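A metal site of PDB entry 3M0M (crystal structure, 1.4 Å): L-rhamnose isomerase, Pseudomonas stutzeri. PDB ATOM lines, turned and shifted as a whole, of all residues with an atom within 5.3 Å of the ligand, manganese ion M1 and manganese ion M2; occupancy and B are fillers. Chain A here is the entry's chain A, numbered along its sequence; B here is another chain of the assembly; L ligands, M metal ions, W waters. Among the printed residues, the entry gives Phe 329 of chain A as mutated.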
ATOM      1  N   TRP A  57      26.451 -22.631  32.080  1.00  0.00           N
ATOM      2  CA  TRP A  57      25.985 -21.444  31.380  1.00  0.00           C
ATOM      3  C   TRP A  57      24.673 -20.874  31.933  1.00  0.00           C
ATOM      4  O   TRP A  57      24.205 -19.837  31.476  1.00  0.00           O
ATOM      5  CB  TRP A  57      25.842 -21.736  29.887  1.00  0.00           C
ATOM      6  CG  TRP A  57      24.855 -22.820  29.540  1.00  0.00           C
ATOM      7  CD1 TRP A  57      23.517 -22.661  29.301  1.00  0.00           C
ATOM      8  CD2 TRP A  57      25.126 -24.214  29.394  1.00  0.00           C
ATOM      9  NE1 TRP A  57      22.945 -23.881  29.002  1.00  0.00           N
ATOM     10  CE2 TRP A  57      23.913 -24.849  29.045  1.00  0.00           C
ATOM     11  CE3 TRP A  57      26.290 -24.997  29.514  1.00  0.00           C
ATOM     12  CZ2 TRP A  57      23.813 -26.232  28.824  1.00  0.00           C
ATOM     13  CZ3 TRP A  57      26.195 -26.371  29.291  1.00  0.00           C
ATOM     14  CH2 TRP A  57      24.964 -26.975  28.949  1.00  0.00           C
ATOM     15  N   HIS A 101      30.751 -26.441  29.214  1.00  0.00           N
ATOM     16  CA  HIS A 101      30.655 -26.059  27.816  1.00  0.00           C
ATOM     17  C   HIS A 101      32.022 -25.508  27.410  1.00  0.00           C
ATOM     18  O   HIS A 101      32.549 -24.609  28.060  1.00  0.00           O
ATOM     19  CB  HIS A 101      29.569 -24.980  27.635  1.00  0.00           C
ATOM     20  CG  HIS A 101      28.799 -25.105  26.355  1.00  0.00           C
ATOM     21  ND1 HIS A 101      29.385 -24.983  25.113  1.00  0.00           N
ATOM     22  CD2 HIS A 101      27.493 -25.343  26.133  1.00  0.00           C
ATOM     23  CE1 HIS A 101      28.468 -25.154  24.176  1.00  0.00           C
ATOM     24  NE2 HIS A 101      27.310 -25.371  24.769  1.00  0.00           N
ATOM     25  N   TRP A 104      33.844 -22.029  26.578  1.00  0.00           N
ATOM     26  CA  TRP A 104      33.428 -21.119  27.651  1.00  0.00           C
ATOM     27  C   TRP A 104      34.088 -21.457  28.977  1.00  0.00           C
ATOM     28  O   TRP A 104      34.598 -20.585  29.677  1.00  0.00           O
ATOM     29  CB  TRP A 104      31.907 -21.127  27.848  1.00  0.00           C
ATOM     30  CG  TRP A 104      31.102 -20.616  26.687  1.00  0.00           C
ATOM     31  CD1 TRP A 104      31.535 -19.835  25.657  1.00  0.00           C
ATOM     32  CD2 TRP A 104      29.714 -20.866  26.456  1.00  0.00           C
ATOM     33  NE1 TRP A 104      30.497 -19.574  24.793  1.00  0.00           N
ATOM     34  CE2 TRP A 104      29.367 -20.194  25.253  1.00  0.00           C
ATOM     35  CE3 TRP A 104      28.724 -21.578  27.141  1.00  0.00           C
ATOM     36  CZ2 TRP A 104      28.067 -20.230  24.731  1.00  0.00           C
ATOM     37  CZ3 TRP A 104      27.432 -21.617  26.617  1.00  0.00           C
ATOM     38  CH2 TRP A 104      27.126 -20.940  25.418  1.00  0.00           C
ATOM     39  N   ASN A 127      29.946 -30.393  26.571  1.00  0.00           N
ATOM     40  CA  ASN A 127      29.233 -29.753  25.477  1.00  0.00           C
ATOM     41  C   ASN A 127      30.240 -29.007  24.610  1.00  0.00           C
ATOM     42  O   ASN A 127      30.985 -28.174  25.117  1.00  0.00           O
ATOM     43  CB  ASN A 127      28.204 -28.755  26.011  1.00  0.00           C
ATOM     44  CG  ASN A 127      27.107 -29.419  26.816  1.00  0.00           C
ATOM     45  OD1 ASN A 127      26.084 -29.840  26.286  1.00  0.00           O
ATOM     46  ND2 ASN A 127      27.328 -29.530  28.124  1.00  0.00           N
ATOM     47  N   SER A 128      30.260 -29.328  23.321  1.00  0.00           N
ATOM     48  CA  SER A 128      31.177 -28.678  22.385  1.00  0.00           C
ATOM     49  C   SER A 128      30.529 -27.406  21.835  1.00  0.00           C
ATOM     50  O   SER A 128      29.317 -27.240  21.901  1.00  0.00           O
ATOM     51  CB  SER A 128      31.523 -29.619  21.234  1.00  0.00           C
ATOM     52  OG  SER A 128      30.350 -30.094  20.605  1.00  0.00           O
ATOM     53  N   PHE A 131      29.391 -23.253  17.158  1.00  0.00           N
ATOM     54  CA  PHE A 131      28.320 -22.390  16.695  1.00  0.00           C
ATOM     55  C   PHE A 131      28.736 -20.926  16.891  1.00  0.00           C
ATOM     56  O   PHE A 131      27.923 -20.007  16.763  1.00  0.00           O
ATOM     57  CB  PHE A 131      27.001 -22.686  17.432  1.00  0.00           C
ATOM     58  CG  PHE A 131      27.115 -22.677  18.944  1.00  0.00           C
ATOM     59  CD1 PHE A 131      27.170 -21.487  19.653  1.00  0.00           C
ATOM     60  CD2 PHE A 131      27.148 -23.877  19.650  1.00  0.00           C
ATOM     61  CE1 PHE A 131      27.242 -21.485  21.041  1.00  0.00           C
ATOM     62  CE2 PHE A 131      27.225 -23.888  21.036  1.00  0.00           C
ATOM     63  CZ  PHE A 131      27.280 -22.690  21.734  1.00  0.00           C
ATOM     64  N   TRP A 179      25.609 -30.020  19.806  1.00  0.00           N
ATOM     65  CA  TRP A 179      24.537 -29.199  19.247  1.00  0.00           C
ATOM     66  C   TRP A 179      25.248 -28.166  18.410  1.00  0.00           C
ATOM     67  O   TRP A 179      26.171 -27.494  18.879  1.00  0.00           O
ATOM     68  CB  TRP A 179      23.714 -28.471  20.308  1.00  0.00           C
ATOM     69  CG  TRP A 179      22.763 -27.499  19.652  1.00  0.00           C
ATOM     70  CD1 TRP A 179      21.619 -27.813  18.953  1.00  0.00           C
ATOM     71  CD2 TRP A 179      22.945 -26.081  19.502  1.00  0.00           C
ATOM     72  NE1 TRP A 179      21.098 -26.689  18.375  1.00  0.00           N
ATOM     73  CE2 TRP A 179      21.882 -25.611  18.698  1.00  0.00           C
ATOM     74  CE3 TRP A 179      23.889 -25.176  19.968  1.00  0.00           C
ATOM     75  CZ2 TRP A 179      21.749 -24.253  18.344  1.00  0.00           C
ATOM     76  CZ3 TRP A 179      23.768 -23.822  19.620  1.00  0.00           C
ATOM     77  CH2 TRP A 179      22.698 -23.384  18.808  1.00  0.00           C
ATOM     78  N   GLU A 219      21.973 -33.345  19.460  1.00  0.00           N
ATOM     79  CA  GLU A 219      20.794 -32.585  19.866  1.00  0.00           C
ATOM     80  C   GLU A 219      20.110 -31.874  18.694  1.00  0.00           C
ATOM     81  O   GLU A 219      20.697 -30.986  18.085  1.00  0.00           O
ATOM     82  CB  GLU A 219      21.204 -31.564  20.929  1.00  0.00           C
ATOM     83  CG  GLU A 219      20.069 -30.734  21.501  1.00  0.00           C
ATOM     84  CD  GLU A 219      20.549 -29.747  22.546  1.00  0.00           C
ATOM     85  OE1 GLU A 219      21.766 -29.655  22.787  1.00  0.00           O
ATOM     86  OE2 GLU A 219      19.695 -29.056  23.134  1.00  0.00           O
ATOM     87  N   LYS A 221      17.220 -29.488  16.709  1.00  0.00           N
ATOM     88  CA  LYS A 221      16.582 -28.194  16.956  1.00  0.00           C
ATOM     89  C   LYS A 221      15.934 -27.734  15.655  1.00  0.00           C
ATOM     90  O   LYS A 221      16.590 -27.688  14.624  1.00  0.00           O
ATOM     91  CB  LYS A 221      17.621 -27.174  17.423  1.00  0.00           C
ATOM     92  CG  LYS A 221      16.992 -25.903  17.958  1.00  0.00           C
ATOM     93  CD  LYS A 221      18.052 -24.905  18.417  1.00  0.00           C
ATOM     94  CE  LYS A 221      17.393 -23.723  19.108  1.00  0.00           C
ATOM     95  NZ  LYS A 221      18.396 -22.696  19.536  1.00  0.00           N
ATOM     96  N   GLU A 224      16.942 -21.682  14.681  1.00  0.00           N
ATOM     97  CA  GLU A 224      17.749 -20.768  15.506  1.00  0.00           C
ATOM     98  C   GLU A 224      19.058 -21.436  15.899  1.00  0.00           C
ATOM     99  O   GLU A 224      19.074 -22.381  16.682  1.00  0.00           O
ATOM    100  CB  GLU A 224      17.019 -20.325  16.773  1.00  0.00           C
ATOM    101  CG  GLU A 224      17.795 -19.208  17.499  1.00  0.00           C
ATOM    102  CD  GLU A 224      17.385 -18.987  18.952  1.00  0.00           C
ATOM    103  OE1 GLU A 224      16.922 -19.943  19.598  1.00  0.00           O
ATOM    104  OE2 GLU A 224      17.562 -17.849  19.438  1.00  0.00           O
ATOM    105  N   LEU A 252      19.547 -36.574  22.084  1.00  0.00           N
ATOM    106  CA  LEU A 252      19.225 -35.753  23.239  1.00  0.00           C
ATOM    107  C   LEU A 252      18.024 -34.885  22.862  1.00  0.00           C
ATOM    108  O   LEU A 252      18.017 -34.242  21.800  1.00  0.00           O
ATOM    109  CB  LEU A 252      20.422 -34.881  23.633  1.00  0.00           C
ATOM    110  CG  LEU A 252      20.211 -34.083  24.915  1.00  0.00           C
ATOM    111  CD1 LEU A 252      21.464 -34.136  25.783  1.00  0.00           C
ATOM    112  CD2 LEU A 252      19.834 -32.653  24.574  1.00  0.00           C
ATOM    113  N   ASP A 254      15.746 -31.732  23.768  1.00  0.00           N
ATOM    114  CA  ASP A 254      15.659 -30.465  24.501  1.00  0.00           C
ATOM    115  C   ASP A 254      14.201 -30.054  24.328  1.00  0.00           C
ATOM    116  O   ASP A 254      13.739 -29.838  23.204  1.00  0.00           O
ATOM    117  CB  ASP A 254      16.601 -29.432  23.882  1.00  0.00           C
ATOM    118  CG  ASP A 254      16.614 -28.113  24.649  1.00  0.00           C
ATOM    119  OD1 ASP A 254      15.512 -27.580  24.910  1.00  0.00           O
ATOM    120  OD2 ASP A 254      17.709 -27.607  24.985  1.00  0.00           O
ATOM    121  N   HIS A 257      12.965 -27.330  21.705  1.00  0.00           N
ATOM    122  CA  HIS A 257      13.479 -27.413  20.335  1.00  0.00           C
ATOM    123  C   HIS A 257      12.512 -28.002  19.298  1.00  0.00           C
ATOM    124  O   HIS A 257      12.959 -28.460  18.235  1.00  0.00           O
ATOM    125  CB  HIS A 257      14.771 -28.242  20.327  1.00  0.00           C
ATOM    126  CG  HIS A 257      15.938 -27.534  20.943  1.00  0.00           C
ATOM    127  ND1 HIS A 257      17.231 -27.976  20.774  1.00  0.00           N
ATOM    128  CD2 HIS A 257      16.014 -26.410  21.699  1.00  0.00           C
ATOM    129  CE1 HIS A 257      18.059 -27.144  21.398  1.00  0.00           C
ATOM    130  NE2 HIS A 257      17.340 -26.194  21.967  1.00  0.00           N
ATOM    131  N   HIS A 281      17.260 -32.209  27.948  1.00  0.00           N
ATOM    132  CA  HIS A 281      17.655 -30.852  28.284  1.00  0.00           C
ATOM    133  C   HIS A 281      16.314 -30.261  28.708  1.00  0.00           C
ATOM    134  O   HIS A 281      15.423 -30.046  27.881  1.00  0.00           O
ATOM    135  CB  HIS A 281      18.237 -30.090  27.084  1.00  0.00           C
ATOM    136  CG  HIS A 281      19.715 -30.203  26.962  1.00  0.00           C
ATOM    137  ND1 HIS A 281      20.462 -29.420  26.115  1.00  0.00           N
ATOM    138  CD2 HIS A 281      20.601 -31.021  27.587  1.00  0.00           C
ATOM    139  CE1 HIS A 281      21.740 -29.747  26.210  1.00  0.00           C
ATOM    140  NE2 HIS A 281      21.851 -30.711  27.106  1.00  0.00           N
ATOM    141  N   ASP A 289      12.411 -21.474  21.447  1.00  0.00           N
ATOM    142  CA  ASP A 289      13.356 -22.090  22.379  1.00  0.00           C
ATOM    143  C   ASP A 289      13.634 -21.033  23.453  1.00  0.00           C
ATOM    144  O   ASP A 289      14.751 -20.542  23.597  1.00  0.00           O
ATOM    145  CB  ASP A 289      14.638 -22.492  21.662  1.00  0.00           C
ATOM    146  CG  ASP A 289      15.623 -23.183  22.579  1.00  0.00           C
ATOM    147  OD1 ASP A 289      15.159 -23.845  23.533  1.00  0.00           O
ATOM    148  OD2 ASP A 289      16.843 -23.068  22.331  1.00  0.00           O
ATOM    149  N   ASP A 291      13.938 -21.158  26.643  1.00  0.00           N
ATOM    150  CA  ASP A 291      14.855 -21.523  27.721  1.00  0.00           C
ATOM    151  C   ASP A 291      14.471 -21.029  29.104  1.00  0.00           C
ATOM    152  O   ASP A 291      15.324 -20.646  29.911  1.00  0.00           O
ATOM    153  CB  ASP A 291      16.276 -21.058  27.382  1.00  0.00           C
ATOM    154  CG  ASP A 291      16.932 -21.944  26.340  1.00  0.00           C
ATOM    155  OD1 ASP A 291      16.758 -23.174  26.450  1.00  0.00           O
ATOM    156  OD2 ASP A 291      17.616 -21.431  25.439  1.00  0.00           O
ATOM    157  N   ASP A 327      18.834 -27.118  30.799  1.00  0.00           N
ATOM    158  CA  ASP A 327      19.439 -26.224  29.814  1.00  0.00           C
ATOM    159  C   ASP A 327      18.537 -25.016  29.782  1.00  0.00           C
ATOM    160  O   ASP A 327      17.501 -25.018  29.106  1.00  0.00           O
ATOM    161  CB  ASP A 327      19.512 -26.853  28.422  1.00  0.00           C
ATOM    162  CG  ASP A 327      20.161 -25.917  27.407  1.00  0.00           C
ATOM    163  OD1 ASP A 327      20.574 -24.809  27.807  1.00  0.00           O
ATOM    164  OD2 ASP A 327      20.267 -26.297  26.224  1.00  0.00           O
ATOM    165  N   PHE A 329      18.364 -20.407  30.411  1.00  0.00           N
ATOM    166  CA  PHE A 329      19.029 -19.115  30.497  1.00  0.00           C
ATOM    167  C   PHE A 329      18.110 -18.275  31.357  1.00  0.00           C
ATOM    168  O   PHE A 329      16.890 -18.327  31.203  1.00  0.00           O
ATOM    169  CB  PHE A 329      19.224 -18.479  29.114  1.00  0.00           C
ATOM    170  CG  PHE A 329      20.362 -19.074  28.342  1.00  0.00           C
ATOM    171  CD1 PHE A 329      20.136 -20.026  27.352  1.00  0.00           C
ATOM    172  CD2 PHE A 329      21.675 -18.723  28.645  1.00  0.00           C
ATOM    173  CE1 PHE A 329      21.202 -20.618  26.663  1.00  0.00           C
ATOM    174  CE2 PHE A 329      22.749 -19.315  27.975  1.00  0.00           C
ATOM    175  CZ  PHE A 329      22.507 -20.271  26.981  1.00  0.00           C
ATOM    176  N   ARG B  65      21.417 -14.630  19.220  1.00  0.00           N
ATOM    177  CA  ARG B  65      21.906 -14.620  20.598  1.00  0.00           C
ATOM    178  C   ARG B  65      23.107 -15.553  20.760  1.00  0.00           C
ATOM    179  O   ARG B  65      23.833 -15.468  21.746  1.00  0.00           O
ATOM    180  CB  ARG B  65      20.809 -15.028  21.582  1.00  0.00           C
ATOM    181  CG  ARG B  65      20.260 -16.416  21.374  1.00  0.00           C
ATOM    182  CD  ARG B  65      19.306 -16.823  22.504  1.00  0.00           C
ATOM    183  NE  ARG B  65      18.559 -18.017  22.125  1.00  0.00           N
ATOM    184  CZ  ARG B  65      18.244 -19.011  22.949  1.00  0.00           C
ATOM    185  NH1 ARG B  65      18.596 -18.984  24.231  1.00  0.00           N
ATOM    186  NH2 ARG B  65      17.574 -20.056  22.481  1.00  0.00           N
ATOM    187  N   PHE B  66      23.331 -16.420  19.777  1.00  0.00           N
ATOM    188  CA  PHE B  66      24.442 -17.362  19.814  1.00  0.00           C
ATOM    189  C   PHE B  66      25.748 -16.827  19.250  1.00  0.00           C
ATOM    190  O   PHE B  66      26.828 -17.157  19.742  1.00  0.00           O
ATOM    191  CB  PHE B  66      24.064 -18.651  19.079  1.00  0.00           C
ATOM    192  CG  PHE B  66      22.994 -19.437  19.778  1.00  0.00           C
ATOM    193  CD1 PHE B  66      23.281 -20.146  20.941  1.00  0.00           C
ATOM    194  CD2 PHE B  66      21.690 -19.427  19.311  1.00  0.00           C
ATOM    195  CE1 PHE B  66      22.286 -20.822  21.629  1.00  0.00           C
ATOM    196  CE2 PHE B  66      20.683 -20.099  19.992  1.00  0.00           C
ATOM    197  CZ  PHE B  66      20.975 -20.799  21.154  1.00  0.00           C
HETATM  198  C1  LIG L   1      20.967 -24.628  21.783  1.00  0.00           C
HETATM  199  O1  LIG L   1      19.908 -24.122  21.388  1.00  0.00           O
HETATM  200  C2  LIG L   1      20.916 -25.933  22.559  1.00  0.00           C
HETATM  201  O2  LIG L   1      19.989 -25.834  23.623  1.00  0.00           O
HETATM  202  C3  LIG L   1      22.300 -26.379  23.067  1.00  0.00           C
HETATM  203  O3  LIG L   1      22.137 -27.326  24.119  1.00  0.00           O
HETATM  204  C4  LIG L   1      23.251 -25.258  23.514  1.00  0.00           C
HETATM  205  O4  LIG L   1      24.583 -25.765  23.493  1.00  0.00           O
HETATM  206  C5  LIG L   1      22.932 -24.753  24.924  1.00  0.00           C
HETATM  207  O5  LIG L   1      21.599 -24.251  24.977  1.00  0.00           O
HETATM  208  C6  LIG L   1      23.909 -23.646  25.306  1.00  0.00           C
HETATM  209  O6  LIG L   1      23.744 -22.532  24.440  1.00  0.00           O
HETATM  210 MN    MN M   1      19.891 -27.714  24.798  1.00  0.00          MN
HETATM  211 MN    MN M   2      18.355 -24.512  22.873  1.00  0.00          MN
HETATM  212  O   HOH W   1      17.258 -24.730  24.534  1.00  0.00           O
HETATM  213  O   HOH W   2      19.355 -23.044  24.008  1.00  0.00           O
HETATM  214  O   HOH W   3      25.130 -28.541  23.880  1.00  0.00           O
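The side-chain amino group (NZ) of Lys 221 sits close to an oxygen (O1) of the ligand (2.8 Å). NE2 of His 101 lies within hydrogen-bond range of O4 of the ligand (3.0 Å).
OD1 of Asp 327 sits at hydrogen-bond distance from NE1 of Trp 57. The side-chain carboxylate (OD2) of Asp 289 lies close to the side-chain amino group (NZ) of Lys 221, at 3.2 Å. O of Asp 289 sits at hydrogen-bond distance from NH2 of Arg 65 of chain B. The side-chain carboxylate (OE1) of Glu 224 is in salt-bridge range of the side-chain amino group (NZ) of Lys 221, 3.1 Å away. The backbone NH (N) of Phe 329 is in hydrogen-bond range of the backbone carbonyl oxygen (O) of Asp 291 (3.1 Å).
Manganese ion M1 is bound by the side-chain carboxylate (OD2) of Asp 327 (2.0 Å), the side-chain carboxylate (OE2) of Glu 219 (2.1 Å), the side-chain carboxylate (OD2) of Asp 254 (2.2 Å), an oxygen (O2) of the ligand (2.2 Å), a ring nitrogen (ND1) of His 281 (2.2 Å) and an oxygen (O3) of the ligand (2.4 Å). Manganese ion M1 has six donor atoms within binding distance.
Residues that only touch manganese ion M2: Lys 221 (3.8 Å). Of the 20 residues printed, 4 come within 4 Å of manganese ion M2.
Trp 57 touches the ligand. Trp 104 touches the ligand. Trp 179 touches the ligand. CZ of Phe 329 touches O6 of the ligand, 3.6 Å away. Phe 66 of chain B touches the ligand (CZ to O1, 3.5 Å). Hydrophobic or aromatic side chains that line the ligand: Trp 57, His 101, Trp 104, Trp 179, His 257, His 281, Phe 329 and Phe 66 of chain B. The nearest printed residue that does not touch the ligand is Phe 131 (4.1 Å).
Water W2 bridges an oxygen (O5) of the ligand (2.7 Å) and the side-chain carboxylate (OD2) of Asp 291 (2.8 Å). Water W3 lies within hydrogen-bond range of O4 of the ligand and OD1 of Asn 127.
Water W1 is bound to manganese ion M2 (2.0 Å). Manganese ion M2 is bound by water W2 (2.1 Å). The side-chain carboxylate (OD2) of Asp 289 is bound to manganese ion M2 (2.2 Å). Manganese ion M2 is bound by a ring nitrogen (NE2) of His 257 (2.2 Å). O1 of the ligand binds manganese ion M2, 2.2 Å away. An oxygen (O2) of the ligand binds manganese ion M2 (2.2 Å). Manganese ion M2 has six donor atoms within binding distance.
Five residues have an atom within 4 Å of manganese ion M1: Glu 219, Asp 254, His 257, His 281 and Asp 327. The nearest printed residue that does not touch manganese ion M1 is Leu 252 (4.9 Å).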
